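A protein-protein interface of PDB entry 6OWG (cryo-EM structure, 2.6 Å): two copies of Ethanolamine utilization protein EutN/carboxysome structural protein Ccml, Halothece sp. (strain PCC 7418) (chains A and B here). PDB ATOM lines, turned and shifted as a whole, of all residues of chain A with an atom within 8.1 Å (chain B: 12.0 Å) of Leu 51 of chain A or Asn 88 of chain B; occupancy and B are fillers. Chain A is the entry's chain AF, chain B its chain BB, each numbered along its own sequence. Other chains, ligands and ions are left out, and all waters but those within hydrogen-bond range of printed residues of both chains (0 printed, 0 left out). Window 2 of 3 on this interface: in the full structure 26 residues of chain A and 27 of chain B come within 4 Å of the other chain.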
ATOM      1  N   LYS A   5       8.566  12.688  -8.439  1.00  0.00           N
ATOM      2  CA  LYS A   5       9.732  13.337  -7.866  1.00  0.00           C
ATOM      3  C   LYS A   5       9.879  12.902  -6.416  1.00  0.00           C
ATOM      4  O   LYS A   5       8.908  12.923  -5.658  1.00  0.00           O
ATOM      5  CB  LYS A   5       9.605  14.857  -7.953  1.00  0.00           C
ATOM      6  CG  LYS A   5      10.854  15.613  -7.582  1.00  0.00           C
ATOM      7  CD  LYS A   5      10.559  17.090  -7.430  1.00  0.00           C
ATOM      8  CE  LYS A   5      11.781  17.852  -6.952  1.00  0.00           C
ATOM      9  NZ  LYS A   5      12.882  17.817  -7.951  1.00  0.00           N
ATOM     10  N   VAL A   6      11.088  12.493  -6.040  1.00  0.00           N
ATOM     11  CA  VAL A   6      11.372  12.060  -4.673  1.00  0.00           C
ATOM     12  C   VAL A   6      11.356  13.303  -3.789  1.00  0.00           C
ATOM     13  O   VAL A   6      12.226  14.165  -3.896  1.00  0.00           O
ATOM     14  CB  VAL A   6      12.703  11.317  -4.567  1.00  0.00           C
ATOM     15  CG1 VAL A   6      12.884  10.764  -3.169  1.00  0.00           C
ATOM     16  CG2 VAL A   6      12.791  10.214  -5.601  1.00  0.00           C
ATOM     17  N   CYS A   7      10.353  13.402  -2.916  1.00  0.00           N
ATOM     18  CA  CYS A   7      10.247  14.565  -2.046  1.00  0.00           C
ATOM     19  C   CYS A   7      10.661  14.248  -0.617  1.00  0.00           C
ATOM     20  O   CYS A   7      10.970  15.162   0.153  1.00  0.00           O
ATOM     21  CB  CYS A   7       8.828  15.127  -2.082  1.00  0.00           C
ATOM     22  SG  CYS A   7       8.442  15.989  -3.618  1.00  0.00           S
ATOM     23  N   GLY A   8      10.678  12.978  -0.238  1.00  0.00           N
ATOM     24  CA  GLY A   8      11.128  12.659   1.091  1.00  0.00           C
ATOM     25  C   GLY A   8      11.082  11.182   1.394  1.00  0.00           C
ATOM     26  O   GLY A   8      10.917  10.347   0.504  1.00  0.00           O
ATOM     27  N   THR A   9      11.241  10.871   2.679  1.00  0.00           N
ATOM     28  CA  THR A   9      11.290   9.504   3.173  1.00  0.00           C
ATOM     29  C   THR A   9      10.221   9.309   4.234  1.00  0.00           C
ATOM     30  O   THR A   9       9.886  10.240   4.969  1.00  0.00           O
ATOM     31  CB  THR A   9      12.667   9.155   3.770  1.00  0.00           C
ATOM     32  OG1 THR A   9      12.954  10.031   4.867  1.00  0.00           O
ATOM     33  CG2 THR A   9      13.762   9.286   2.734  1.00  0.00           C
ATOM     34  N   LYS A  23      12.863   0.160   1.873  1.00  0.00           N
ATOM     35  CA  LYS A  23      13.064   1.600   1.920  1.00  0.00           C
ATOM     36  C   LYS A  23      11.852   2.286   1.304  1.00  0.00           C
ATOM     37  O   LYS A  23      11.460   1.970   0.178  1.00  0.00           O
ATOM     38  CB  LYS A  23      14.347   1.973   1.182  1.00  0.00           C
ATOM     39  CG  LYS A  23      14.515   3.447   0.897  1.00  0.00           C
ATOM     40  CD  LYS A  23      15.642   3.664  -0.094  1.00  0.00           C
ATOM     41  CE  LYS A  23      15.756   5.118  -0.496  1.00  0.00           C
ATOM     42  NZ  LYS A  23      16.630   5.294  -1.684  1.00  0.00           N
ATOM     43  N   LEU A  25       9.983   5.690   0.090  1.00  0.00           N
ATOM     44  CA  LEU A  25      10.160   7.055  -0.373  1.00  0.00           C
ATOM     45  C   LEU A  25       8.811   7.730  -0.553  1.00  0.00           C
ATOM     46  O   LEU A  25       7.865   7.153  -1.085  1.00  0.00           O
ATOM     47  CB  LEU A  25      10.938   7.084  -1.690  1.00  0.00           C
ATOM     48  CG  LEU A  25      12.434   6.806  -1.624  1.00  0.00           C
ATOM     49  CD1 LEU A  25      13.038   7.008  -2.986  1.00  0.00           C
ATOM     50  CD2 LEU A  25      13.088   7.717  -0.616  1.00  0.00           C
ATOM     51  N   LEU A  26       8.737   8.978  -0.109  1.00  0.00           N
ATOM     52  CA  LEU A  26       7.588   9.835  -0.364  1.00  0.00           C
ATOM     53  C   LEU A  26       7.807  10.505  -1.713  1.00  0.00           C
ATOM     54  O   LEU A  26       8.697  11.349  -1.854  1.00  0.00           O
ATOM     55  CB  LEU A  26       7.412  10.867   0.745  1.00  0.00           C
ATOM     56  CG  LEU A  26       6.182  11.757   0.605  1.00  0.00           C
ATOM     57  CD1 LEU A  26       4.951  11.019   1.073  1.00  0.00           C
ATOM     58  CD2 LEU A  26       6.367  13.041   1.379  1.00  0.00           C
ATOM     59  N   GLY A  48      18.250   2.729  -6.006  1.00  0.00           N
ATOM     60  CA  GLY A  48      18.524   3.686  -4.944  1.00  0.00           C
ATOM     61  C   GLY A  48      18.368   5.125  -5.392  1.00  0.00           C
ATOM     62  O   GLY A  48      19.216   5.650  -6.131  1.00  0.00           O
ATOM     63  N   ALA A  49      17.303   5.782  -4.940  1.00  0.00           N
ATOM     64  CA  ALA A  49      16.926   7.107  -5.407  1.00  0.00           C
ATOM     65  C   ALA A  49      16.939   8.081  -4.242  1.00  0.00           C
ATOM     66  O   ALA A  49      16.408   7.781  -3.168  1.00  0.00           O
ATOM     67  CB  ALA A  49      15.542   7.085  -6.059  1.00  0.00           C
ATOM     68  N   GLY A  50      17.543   9.247  -4.459  1.00  0.00           N
ATOM     69  CA  GLY A  50      17.636  10.267  -3.443  1.00  0.00           C
ATOM     70  C   GLY A  50      16.692  11.426  -3.706  1.00  0.00           C
ATOM     71  O   GLY A  50      15.982  11.476  -4.705  1.00  0.00           O
ATOM     72  N   LEU A  51      16.724  12.381  -2.784  1.00  0.00           N
ATOM     73  CA  LEU A  51      15.750  13.461  -2.772  1.00  0.00           C
ATOM     74  C   LEU A  51      15.984  14.423  -3.928  1.00  0.00           C
ATOM     75  O   LEU A  51      17.083  14.951  -4.111  1.00  0.00           O
ATOM     76  CB  LEU A  51      15.822  14.197  -1.437  1.00  0.00           C
ATOM     77  CG  LEU A  51      14.633  15.055  -1.021  1.00  0.00           C
ATOM     78  CD1 LEU A  51      14.396  14.849   0.452  1.00  0.00           C
ATOM     79  CD2 LEU A  51      14.892  16.518  -1.307  1.00  0.00           C
ATOM     80  N   GLY A  52      14.931  14.646  -4.711  1.00  0.00           N
ATOM     81  CA  GLY A  52      14.991  15.498  -5.871  1.00  0.00           C
ATOM     82  C   GLY A  52      15.008  14.774  -7.197  1.00  0.00           C
ATOM     83  O   GLY A  52      14.810  15.417  -8.234  1.00  0.00           O
ATOM     84  N   GLU A  53      15.234  13.465  -7.201  1.00  0.00           N
ATOM     85  CA  GLU A  53      15.334  12.723  -8.446  1.00  0.00           C
ATOM     86  C   GLU A  53      13.966  12.498  -9.067  1.00  0.00           C
ATOM     87  O   GLU A  53      12.939  12.506  -8.386  1.00  0.00           O
ATOM     88  CB  GLU A  53      15.996  11.366  -8.229  1.00  0.00           C
ATOM     89  CG  GLU A  53      17.427  11.409  -7.767  1.00  0.00           C
ATOM     90  CD  GLU A  53      18.027  10.025  -7.718  1.00  0.00           C
ATOM     91  OE1 GLU A  53      17.305   9.072  -8.064  1.00  0.00           O
ATOM     92  OE2 GLU A  53      19.199   9.880  -7.317  1.00  0.00           O
ATOM     93  N   TRP A  54      13.967  12.284 -10.375  1.00  0.00           N
ATOM     94  CA  TRP A  54      12.783  11.881 -11.115  1.00  0.00           C
ATOM     95  C   TRP A  54      12.793  10.368 -11.250  1.00  0.00           C
ATOM     96  O   TRP A  54      13.785   9.789 -11.696  1.00  0.00           O
ATOM     97  CB  TRP A  54      12.752  12.533 -12.494  1.00  0.00           C
ATOM     98  CG  TRP A  54      12.298  13.944 -12.486  1.00  0.00           C
ATOM     99  CD1 TRP A  54      12.440  14.849 -11.478  1.00  0.00           C
ATOM    100  CD2 TRP A  54      11.629  14.625 -13.546  1.00  0.00           C
ATOM    101  NE1 TRP A  54      11.896  16.052 -11.844  1.00  0.00           N
ATOM    102  CE2 TRP A  54      11.391  15.942 -13.111  1.00  0.00           C
ATOM    103  CE3 TRP A  54      11.199  14.246 -14.822  1.00  0.00           C
ATOM    104  CZ2 TRP A  54      10.744  16.881 -13.905  1.00  0.00           C
ATOM    105  CZ3 TRP A  54      10.555  15.179 -15.604  1.00  0.00           C
ATOM    106  CH2 TRP A  54      10.337  16.481 -15.146  1.00  0.00           C
ATOM    107  N   MET B   3      -0.331   7.518   2.807  1.00  0.00           N
ATOM    108  CA  MET B   3      -0.361   7.936   4.196  1.00  0.00           C
ATOM    109  C   MET B   3      -1.794   8.265   4.580  1.00  0.00           C
ATOM    110  O   MET B   3      -2.504   8.954   3.846  1.00  0.00           O
ATOM    111  CB  MET B   3       0.539   9.148   4.425  1.00  0.00           C
ATOM    112  CG  MET B   3       2.000   8.891   4.134  1.00  0.00           C
ATOM    113  SD  MET B   3       3.074  10.158   4.813  1.00  0.00           S
ATOM    114  CE  MET B   3       2.456  11.610   3.977  1.00  0.00           C
ATOM    115  N   ALA B  32       0.828  14.853   1.121  1.00  0.00           N
ATOM    116  CA  ALA B  32       2.258  14.877   1.399  1.00  0.00           C
ATOM    117  C   ALA B  32       2.643  16.059   2.278  1.00  0.00           C
ATOM    118  O   ALA B  32       3.713  16.046   2.896  1.00  0.00           O
ATOM    119  CB  ALA B  32       3.045  14.910   0.091  1.00  0.00           C
ATOM    120  N   ASN B  33       1.794  17.087   2.344  1.00  0.00           N
ATOM    121  CA  ASN B  33       2.085  18.240   3.187  1.00  0.00           C
ATOM    122  C   ASN B  33       1.542  18.060   4.601  1.00  0.00           C
ATOM    123  O   ASN B  33       1.949  18.789   5.513  1.00  0.00           O
ATOM    124  CB  ASN B  33       1.511  19.503   2.550  1.00  0.00           C
ATOM    125  CG  ASN B  33       2.125  19.806   1.199  1.00  0.00           C
ATOM    126  OD1 ASN B  33       1.453  19.732   0.171  1.00  0.00           O
ATOM    127  ND2 ASN B  33       3.405  20.155   1.194  1.00  0.00           N
ATOM    128  N   GLY B  34       0.624  17.119   4.804  1.00  0.00           N
ATOM    129  CA  GLY B  34       0.120  16.804   6.125  1.00  0.00           C
ATOM    130  C   GLY B  34      -1.346  17.094   6.382  1.00  0.00           C
ATOM    131  O   GLY B  34      -1.840  16.751   7.462  1.00  0.00           O
ATOM    132  N   THR B  84       8.084   8.529  11.393  1.00  0.00           N
ATOM    133  CA  THR B  84       8.642   9.810  10.988  1.00  0.00           C
ATOM    134  C   THR B  84       8.418  10.014   9.498  1.00  0.00           C
ATOM    135  O   THR B  84       8.681   9.115   8.699  1.00  0.00           O
ATOM    136  CB  THR B  84      10.144   9.882  11.303  1.00  0.00           C
ATOM    137  OG1 THR B  84      10.365   9.592  12.688  1.00  0.00           O
ATOM    138  CG2 THR B  84      10.702  11.260  10.996  1.00  0.00           C
ATOM    139  N   VAL B  85       7.923  11.194   9.134  1.00  0.00           N
ATOM    140  CA  VAL B  85       7.910  11.655   7.751  1.00  0.00           C
ATOM    141  C   VAL B  85       8.873  12.823   7.643  1.00  0.00           C
ATOM    142  O   VAL B  85       8.691  13.849   8.306  1.00  0.00           O
ATOM    143  CB  VAL B  85       6.504  12.071   7.285  1.00  0.00           C
ATOM    144  CG1 VAL B  85       6.554  12.556   5.853  1.00  0.00           C
ATOM    145  CG2 VAL B  85       5.561  10.918   7.394  1.00  0.00           C
ATOM    146  N   THR B  86       9.902  12.660   6.823  1.00  0.00           N
ATOM    147  CA  THR B  86      10.875  13.710   6.555  1.00  0.00           C
ATOM    148  C   THR B  86      10.681  14.161   5.119  1.00  0.00           C
ATOM    149  O   THR B  86      10.802  13.351   4.199  1.00  0.00           O
ATOM    150  CB  THR B  86      12.301  13.205   6.778  1.00  0.00           C
ATOM    151  OG1 THR B  86      12.406  12.634   8.089  1.00  0.00           O
ATOM    152  CG2 THR B  86      13.292  14.336   6.656  1.00  0.00           C
ATOM    153  N   VAL B  87      10.350  15.435   4.927  1.00  0.00           N
ATOM    154  CA  VAL B  87      10.153  16.015   3.602  1.00  0.00           C
ATOM    155  C   VAL B  87      11.171  17.128   3.419  1.00  0.00           C
ATOM    156  O   VAL B  87      11.206  18.070   4.222  1.00  0.00           O
ATOM    157  CB  VAL B  87       8.728  16.556   3.410  1.00  0.00           C
ATOM    158  CG1 VAL B  87       8.513  16.961   1.968  1.00  0.00           C
ATOM    159  CG2 VAL B  87       7.697  15.534   3.834  1.00  0.00           C
ATOM    160  N   ASN B  88      11.983  17.018   2.356  1.00  0.00           N
ATOM    161  CA  ASN B  88      13.029  17.988   1.996  1.00  0.00           C
ATOM    162  C   ASN B  88      14.024  18.189   3.138  1.00  0.00           C
ATOM    163  O   ASN B  88      14.373  19.318   3.490  1.00  0.00           O
ATOM    164  CB  ASN B  88      12.426  19.323   1.544  1.00  0.00           C
ATOM    165  CG  ASN B  88      13.339  20.093   0.616  1.00  0.00           C
ATOM    166  OD1 ASN B  88      14.262  19.534   0.028  1.00  0.00           O
ATOM    167  ND2 ASN B  88      13.087  21.388   0.483  1.00  0.00           N
ATOM    168  N   ASN B  89      14.448  17.074   3.740  1.00  0.00           N
ATOM    169  CA  ASN B  89      15.317  16.968   4.914  1.00  0.00           C
ATOM    170  C   ASN B  89      14.756  17.665   6.148  1.00  0.00           C
ATOM    171  O   ASN B  89      15.508  17.944   7.088  1.00  0.00           O
ATOM    172  CB  ASN B  89      16.737  17.478   4.634  1.00  0.00           C
ATOM    173  CG  ASN B  89      17.412  16.726   3.509  1.00  0.00           C
ATOM    174  OD1 ASN B  89      17.870  17.322   2.536  1.00  0.00           O
ATOM    175  ND2 ASN B  89      17.472  15.406   3.632  1.00  0.00           N
ATOM    176  N   ARG B  90      13.455  17.939   6.181  1.00  0.00           N
ATOM    177  CA  ARG B  90      12.786  18.547   7.320  1.00  0.00           C
ATOM    178  C   ARG B  90      11.737  17.573   7.830  1.00  0.00           C
ATOM    179  O   ARG B  90      10.957  17.033   7.041  1.00  0.00           O
ATOM    180  CB  ARG B  90      12.141  19.880   6.933  1.00  0.00           C
ATOM    181  CG  ARG B  90      11.261  20.483   8.010  1.00  0.00           C
ATOM    182  CD  ARG B  90      10.814  21.891   7.658  1.00  0.00           C
ATOM    183  NE  ARG B  90       9.747  21.903   6.661  1.00  0.00           N
ATOM    184  CZ  ARG B  90       8.452  21.831   6.952  1.00  0.00           C
ATOM    185  NH1 ARG B  90       7.551  21.852   5.980  1.00  0.00           N
ATOM    186  NH2 ARG B  90       8.057  21.735   8.214  1.00  0.00           N
ATOM    187  N   ARG B  91      11.729  17.341   9.140  1.00  0.00           N
ATOM    188  CA  ARG B  91      10.781  16.412   9.735  1.00  0.00           C
ATOM    189  C   ARG B  91       9.376  17.000   9.708  1.00  0.00           C
ATOM    190  O   ARG B  91       9.122  18.053  10.299  1.00  0.00           O
ATOM    191  CB  ARG B  91      11.195  16.081  11.165  1.00  0.00           C
ATOM    192  CG  ARG B  91      10.161  15.286  11.929  1.00  0.00           C
ATOM    193  CD  ARG B  91      10.746  14.673  13.183  1.00  0.00           C
ATOM    194  NE  ARG B  91      11.901  13.832  12.891  1.00  0.00           N
ATOM    195  CZ  ARG B  91      12.394  12.927  13.728  1.00  0.00           C
ATOM    196  NH1 ARG B  91      11.831  12.739  14.912  1.00  0.00           N
ATOM    197  NH2 ARG B  91      13.450  12.205  13.377  1.00  0.00           N
ATOM    198  N   LEU B  92       8.470  16.321   9.008  1.00  0.00           N
ATOM    199  CA  LEU B  92       7.064  16.695   8.951  1.00  0.00           C
ATOM    200  C   LEU B  92       6.246  16.084  10.074  1.00  0.00           C
ATOM    201  O   LEU B  92       5.373  16.756  10.631  1.00  0.00           O
ATOM    202  CB  LEU B  92       6.461  16.263   7.610  1.00  0.00           C
ATOM    203  CG  LEU B  92       5.001  16.632   7.344  1.00  0.00           C
ATOM    204  CD1 LEU B  92       4.841  18.137   7.203  1.00  0.00           C
ATOM    205  CD2 LEU B  92       4.466  15.902   6.129  1.00  0.00           C
ATOM    206  N   TYR B  93       6.524  14.835  10.426  1.00  0.00           N
ATOM    207  CA  TYR B  93       5.772  14.108  11.434  1.00  0.00           C
ATOM    208  C   TYR B  93       6.747  13.369  12.335  1.00  0.00           C
ATOM    209  O   TYR B  93       7.793  12.900  11.885  1.00  0.00           O
ATOM    210  CB  TYR B  93       4.793  13.127  10.782  1.00  0.00           C
ATOM    211  CG  TYR B  93       3.907  12.380  11.748  1.00  0.00           C
ATOM    212  CD1 TYR B  93       2.831  13.009  12.358  1.00  0.00           C
ATOM    213  CD2 TYR B  93       4.139  11.044  12.039  1.00  0.00           C
ATOM    214  CE1 TYR B  93       2.018  12.328  13.238  1.00  0.00           C
ATOM    215  CE2 TYR B  93       3.332  10.357  12.917  1.00  0.00           C
ATOM    216  CZ  TYR B  93       2.273  11.004  13.513  1.00  0.00           C
ATOM    217  OH  TYR B  93       1.462  10.320  14.386  1.00  0.00           O
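The side-chain sulfur of Cys 7 of chain A is in hydrogen-bond range of the backbone carbonyl oxygen of Lys 5 of chain A (3.7 Å). The backbone NH of Cys 7 of chain A is in hydrogen-bond range of the backbone carbonyl oxygen of Leu 26 of chain A (2.8 Å). The backbone NH (N) of Leu 26 of chain A sits at hydrogen-bond distance from the backbone carbonyl oxygen (O) of Gly 8 of chain A, at 2.6 Å. The backbone carbonyl oxygen (O) of Val 85 of chain B is in hydrogen-bond range of the backbone NH (N) of Leu 92 of chain B (2.6 Å). O of Val 85 of chain B sits at hydrogen-bond distance from N of Tyr 93 of chain B.
Of chain B, only Asn 88 (3.4 Å) and Asn 89 (3.97 Å) come within 4 Å of Leu 51 of chain A. No residue of chain B comes within 4 Å of Val 6 of chain A. Cys 7 of chain A touches two residues of chain B. Gly 8 of chain A touches one residue of chain B. Gly 52 of chain A touches none of the printed residues of chain B. No residue of chain B comes within 4 Å of Glu 53 of chain A. Printed residues of chain B within 4 Å of Leu 26 of chain A: Met 3 and Val 87. Printed residues of chain A within 4 Å of Thr 86 of chain B: Gly 8 (3.2 Å) and Thr 9 (2.9 Å). Arg 91 of chain B touches none of the printed residues of chain A. Arg 90 of chain B touches none of the printed residues of chain A. The nearest residue of chain B that does not touch Leu 51 of chain A is Val 87 of chain B (4.9 Å). The nearest residue of chain A that does not touch Asn 88 of chain B is Gly 8 of chain A (4.6 Å). The nearest printed residue of chain B that does not touch Leu 26 of chain A is Ala 32 of chain B (4.02 Å).
The backbone NH of Asn 88 of chain B sits at hydrogen-bond distance from the backbone carbonyl oxygen of Cys 7 of chain A, 3.1 Å away. The backbone carbonyl oxygen of Thr 86 of chain B sits at hydrogen-bond distance from the backbone NH of Thr 9 of chain A, at 2.9 Å.
Hydrophobic or aromatic side chains of chain A within 4 Å of the printed part of chain B: Leu 26 and Leu 51. Of the 14 printed residues of chain B, 6 touch a printed residue of chain A. Printed residues of chain B that touch a printed residue of chain A: Met 3, Val 85, Thr 86, Val 87, Asn 88 and Asn 89. Among the printed residues, no Asp or Glu carboxylate lies within 4 Å of a Lys or Arg side-chain nitrogen of the other chain.
No position is printed for both chains. Of the 9 pairs that touch across the chains among the printed residues, none has its exchanged pair printed and touching as well.
Among the printed residues, pairs that only touch across the chains: Gly 8 of chain A with Thr 86 of chain B, Leu 51 of chain A with Asn 88 of chain B, Cys 7 of chain A with Val 87 of chain B, Thr 9 of chain A with Val 85 of chain B, Leu 26 of chain A with Val 87 of chain B, Leu 26 of chain A with Met 3 of chain B and Leu 51 of chain A with Asn 89 of chain B.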
